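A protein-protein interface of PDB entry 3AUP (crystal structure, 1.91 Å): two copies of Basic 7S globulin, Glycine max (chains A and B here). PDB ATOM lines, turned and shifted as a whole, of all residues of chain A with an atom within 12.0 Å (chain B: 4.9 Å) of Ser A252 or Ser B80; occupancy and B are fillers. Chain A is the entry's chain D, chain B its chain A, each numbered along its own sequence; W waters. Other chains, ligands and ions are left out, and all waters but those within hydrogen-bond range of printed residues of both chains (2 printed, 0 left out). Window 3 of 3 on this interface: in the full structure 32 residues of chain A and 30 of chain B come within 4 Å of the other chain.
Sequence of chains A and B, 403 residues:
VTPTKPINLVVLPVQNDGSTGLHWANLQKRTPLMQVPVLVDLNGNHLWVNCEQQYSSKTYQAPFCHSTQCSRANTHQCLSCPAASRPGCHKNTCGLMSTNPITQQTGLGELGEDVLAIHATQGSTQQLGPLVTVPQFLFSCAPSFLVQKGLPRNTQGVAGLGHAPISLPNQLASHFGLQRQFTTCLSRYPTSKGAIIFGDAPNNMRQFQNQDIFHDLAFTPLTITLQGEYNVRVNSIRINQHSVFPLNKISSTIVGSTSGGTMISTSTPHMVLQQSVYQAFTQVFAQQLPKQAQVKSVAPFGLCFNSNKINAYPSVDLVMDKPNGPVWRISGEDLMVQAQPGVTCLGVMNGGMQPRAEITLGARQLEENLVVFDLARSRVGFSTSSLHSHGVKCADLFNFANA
The backbone carbonyl oxygen of Cys B78 lies within hydrogen-bond range of the backbone NH of Val A255 (3.2 Å).
The backbone NH of Ser B80 sits at hydrogen-bond distance from the backbone carbonyl oxygen of Thr A253 (2.8 Å).
The backbone NH (N) of Asn B92 lies within hydrogen-bond range of the backbone carbonyl oxygen (O) of Leu B79 (3.1 Å).
Among the printed residues, merely in contact across the chains: Ser A252 with Leu B79, Ser A252 with Ser B80, Ser A252 with Leu B108, Thr A253 with Leu B79, Ile A254 with Cys B78, Ile A254 with Leu B79 and Ser A257 with Cys B78.
Ser A252 touches just these residues of chain B: Leu B79 (3.2 Å), Ser B80 (3.7 Å) and Leu B108 (3.7 Å).
Printed residues of chain B within 4 Å of Thr A253: Leu B79 and Ser B80.
Printed residues of chain B within 4 Å of Ile A254: Cys B78 (3.7 Å) and Leu B79 (3.8 Å).
Printed residues of chain B within 4 Å of Val A255: Cys B78 (3.2 Å).
Printed residues of chain B within 4 Å of Ser A257: Cys B78 (3.9 Å).
Of chain A, only Ile A254, Val A255 and Ser A257 come within 4 Å of Cys B78.
Of the printed residues of chain A, Leu B79 touches Ser A252 (3.2 Å), Thr A253 (3.1 Å) and Ile A254 (3.8 Å).
Of chain A, only Ser A252 and Thr A253 come within 4 Å of Ser B80.
Pro B82 touches none of the printed residues of chain A.
Gly B88 touches none of the printed residues of chain A.
No residue of chain A comes within 4 Å of Lys B91.
Of chain A, only Ser A252 (3.7 Å) comes within 4 Å of Leu B108.
The nearest printed residue of chain B that does not touch Ser A257 is Asn B92 (4.1 Å).
Hydrophobic or aromatic side chains of chain B that line the printed part of chain A: Leu B79 and Leu B108.
Of the 6 printed residues of chain A, 5 touch a printed residue of chain B.
Hydrophobic or aromatic side chains of chain A that line the printed part of chain B: Ile A254.
Along chain A the printed residues that touch a printed residue of chain B span positions 252 to 257.
Among the printed residues, 9 pairs touch across the chains.
No position is printed for both chains.
Of the 9 pairs that touch across the chains among the printed residues, none has its exchanged pair printed and touching as well.
Water W1 lies within hydrogen-bond range of N of Ser A252 and SG of Cys B81.
Water W2 bridges N of Cys B78 (2.8 Å) and N of Gly A256 (3.4 Å).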
ATOM      1  N   SER A 252       8.613  -3.917  26.701  1.00  0.00           N
ATOM      2  CA  SER A 252       7.818  -2.843  26.089  1.00  0.00           C
ATOM      3  C   SER A 252       6.461  -2.543  26.794  1.00  0.00           C
ATOM      4  O   SER A 252       5.425  -2.476  26.126  1.00  0.00           O
ATOM      5  CB  SER A 252       7.630  -3.101  24.582  1.00  0.00           C
ATOM      6  OG  SER A 252       6.730  -4.138  24.311  1.00  0.00           O
ATOM      7  N   THR A 253       6.493  -2.380  28.132  1.00  0.00           N
ATOM      8  CA  THR A 253       5.503  -1.571  28.864  1.00  0.00           C
ATOM      9  C   THR A 253       5.581  -0.111  28.372  1.00  0.00           C
ATOM     10  O   THR A 253       6.661   0.387  28.039  1.00  0.00           O
ATOM     11  CB  THR A 253       5.754  -1.595  30.409  1.00  0.00           C
ATOM     12  OG1 THR A 253       4.778  -2.402  31.067  1.00  0.00           O
ATOM     13  CG2 THR A 253       5.700  -0.193  31.006  1.00  0.00           C
ATOM     14  N   ILE A 254       4.441   0.571  28.327  1.00  0.00           N
ATOM     15  CA  ILE A 254       4.404   1.972  27.922  1.00  0.00           C
ATOM     16  C   ILE A 254       4.588   2.851  29.153  1.00  0.00           C
ATOM     17  O   ILE A 254       4.036   2.528  30.204  1.00  0.00           O
ATOM     18  CB  ILE A 254       3.084   2.293  27.189  1.00  0.00           C
ATOM     19  CG1 ILE A 254       3.186   1.739  25.782  1.00  0.00           C
ATOM     20  CG2 ILE A 254       2.826   3.812  27.160  1.00  0.00           C
ATOM     21  CD1 ILE A 254       1.907   1.308  25.226  1.00  0.00           C
ATOM     22  N   VAL A 255       5.380   3.926  29.022  1.00  0.00           N
ATOM     23  CA  VAL A 255       5.724   4.821  30.153  1.00  0.00           C
ATOM     24  C   VAL A 255       5.052   6.224  30.110  1.00  0.00           C
ATOM     25  O   VAL A 255       4.094   6.503  30.857  1.00  0.00           O
ATOM     26  CB  VAL A 255       7.270   5.034  30.249  1.00  0.00           C
ATOM     27  N   GLY A 256       5.603   7.116  29.285  1.00  0.00           N
ATOM     28  CA  GLY A 256       5.043   8.458  29.075  1.00  0.00           C
ATOM     29  C   GLY A 256       5.754   9.672  29.654  1.00  0.00           C
ATOM     30  O   GLY A 256       5.299  10.266  30.642  1.00  0.00           O
ATOM     31  N   SER A 257       6.809  10.093  28.973  1.00  0.00           N
ATOM     32  CA  SER A 257       7.771  11.041  29.508  1.00  0.00           C
ATOM     33  C   SER A 257       7.818  12.343  28.702  1.00  0.00           C
ATOM     34  O   SER A 257       6.950  12.613  27.881  1.00  0.00           O
ATOM     35  CB  SER A 257       9.129  10.353  29.491  1.00  0.00           C
ATOM     36  OG  SER A 257       8.948   8.952  29.680  1.00  0.00           O
ATOM     37  N   CYS B  78       7.148   6.038  24.316  1.00  0.00           N
ATOM     38  CA  CYS B  78       8.270   5.624  25.174  1.00  0.00           C
ATOM     39  C   CYS B  78       7.968   4.266  25.763  1.00  0.00           C
ATOM     40  O   CYS B  78       6.847   4.061  26.159  1.00  0.00           O
ATOM     41  CB  CYS B  78       8.388   6.601  26.335  1.00  0.00           C
ATOM     42  SG  CYS B  78       8.768   8.332  25.883  1.00  0.00           S
ATOM     43  N   LEU B  79       8.965   3.395  25.903  1.00  0.00           N
ATOM     44  CA  LEU B  79       8.786   2.074  26.477  1.00  0.00           C
ATOM     45  C   LEU B  79       9.763   1.786  27.576  1.00  0.00           C
ATOM     46  O   LEU B  79      10.860   2.338  27.606  1.00  0.00           O
ATOM     47  CB  LEU B  79       9.027   0.946  25.468  1.00  0.00           C
ATOM     48  CG  LEU B  79       8.161   0.948  24.268  1.00  0.00           C
ATOM     49  CD1 LEU B  79       8.513  -0.280  23.431  1.00  0.00           C
ATOM     50  CD2 LEU B  79       6.719   0.964  24.702  1.00  0.00           C
ATOM     51  N   SER B  80       9.355   0.879  28.453  1.00  0.00           N
ATOM     52  CA  SER B  80      10.256   0.339  29.451  1.00  0.00           C
ATOM     53  C   SER B  80       9.986  -1.140  29.700  1.00  0.00           C
ATOM     54  O   SER B  80       8.870  -1.617  29.528  1.00  0.00           O
ATOM     55  CB  SER B  80      10.104   1.091  30.752  1.00  0.00           C
ATOM     56  OG  SER B  80       8.875   0.726  31.354  1.00  0.00           O
ATOM     57  N   CYS B  81      11.031  -1.849  30.113  1.00  0.00           N
ATOM     58  CA  CYS B  81      10.980  -3.278  30.321  1.00  0.00           C
ATOM     59  C   CYS B  81      11.369  -3.525  31.775  1.00  0.00           C
ATOM     60  O   CYS B  81      12.340  -2.939  32.258  1.00  0.00           O
ATOM     61  CB  CYS B  81      11.975  -3.920  29.385  1.00  0.00           C
ATOM     62  SG  CYS B  81      12.014  -5.688  29.389  1.00  0.00           S
ATOM     63  N   PRO B  82      10.593  -4.357  32.483  1.00  0.00           N
ATOM     64  CA  PRO B  82      10.887  -4.653  33.874  1.00  0.00           C
ATOM     65  C   PRO B  82      11.781  -5.865  33.959  1.00  0.00           C
ATOM     66  O   PRO B  82      11.297  -6.982  34.205  1.00  0.00           O
ATOM     67  CB  PRO B  82       9.510  -4.980  34.451  1.00  0.00           C
ATOM     68  CG  PRO B  82       8.813  -5.669  33.318  1.00  0.00           C
ATOM     69  CD  PRO B  82       9.295  -4.930  32.067  1.00  0.00           C
ATOM     70  N   GLY B  88      16.042  -5.564  23.012  1.00  0.00           N
ATOM     71  CA  GLY B  88      14.597  -5.747  23.144  1.00  0.00           C
ATOM     72  C   GLY B  88      13.960  -5.337  24.461  1.00  0.00           C
ATOM     73  O   GLY B  88      12.725  -5.306  24.564  1.00  0.00           O
ATOM     74  N   HIS B  90      14.747  -2.574  27.649  1.00  0.00           N
ATOM     75  CA  HIS B  90      15.498  -1.474  28.247  1.00  0.00           C
ATOM     76  C   HIS B  90      14.560  -0.563  29.024  1.00  0.00           C
ATOM     77  O   HIS B  90      13.326  -0.675  28.927  1.00  0.00           O
ATOM     78  CB  HIS B  90      16.184  -0.651  27.169  1.00  0.00           C
ATOM     79  CG  HIS B  90      17.251  -1.375  26.408  1.00  0.00           C
ATOM     80  ND1 HIS B  90      17.012  -2.024  25.215  1.00  0.00           N
ATOM     81  CD2 HIS B  90      18.583  -1.503  26.645  1.00  0.00           C
ATOM     82  CE1 HIS B  90      18.141  -2.540  24.766  1.00  0.00           C
ATOM     83  NE2 HIS B  90      19.106  -2.248  25.618  1.00  0.00           N
ATOM     84  N   LYS B  91      15.146   0.346  29.793  1.00  0.00           N
ATOM     85  CA  LYS B  91      14.390   1.426  30.415  1.00  0.00           C
ATOM     86  C   LYS B  91      14.431   2.623  29.447  1.00  0.00           C
ATOM     87  O   LYS B  91      15.464   2.901  28.867  1.00  0.00           O
ATOM     88  CB  LYS B  91      14.998   1.790  31.770  1.00  0.00           C
ATOM     89  N   ASN B  92      13.306   3.295  29.234  1.00  0.00           N
ATOM     90  CA  ASN B  92      13.284   4.530  28.425  1.00  0.00           C
ATOM     91  C   ASN B  92      13.730   4.472  26.944  1.00  0.00           C
ATOM     92  O   ASN B  92      14.603   5.242  26.499  1.00  0.00           O
ATOM     93  CB  ASN B  92      14.072   5.632  29.143  1.00  0.00           C
ATOM     94  CG  ASN B  92      13.688   7.013  28.656  1.00  0.00           C
ATOM     95  OD1 ASN B  92      12.490   7.292  28.442  1.00  0.00           O
ATOM     96  ND2 ASN B  92      14.699   7.891  28.451  1.00  0.00           N
ATOM     97  N   LEU B 108       3.951  -4.627  18.961  1.00  0.00           N
ATOM     98  CA  LEU B 108       4.709  -3.552  19.488  1.00  0.00           C
ATOM     99  C   LEU B 108       6.143  -4.017  19.870  1.00  0.00           C
ATOM    100  O   LEU B 108       6.309  -4.924  20.683  1.00  0.00           O
ATOM    101  CB  LEU B 108       3.963  -2.958  20.709  1.00  0.00           C
ATOM    102  CG  LEU B 108       4.709  -1.790  21.404  1.00  0.00           C
ATOM    103  CD1 LEU B 108       4.945  -0.570  20.540  1.00  0.00           C
ATOM    104  CD2 LEU B 108       4.024  -1.430  22.721  1.00  0.00           C
HETATM  105  O   HOH W   1       9.014  -5.756  28.237  1.00  0.00           O
HETATM  106  O   HOH W   2       5.041   6.972  25.905  1.00  0.00           O
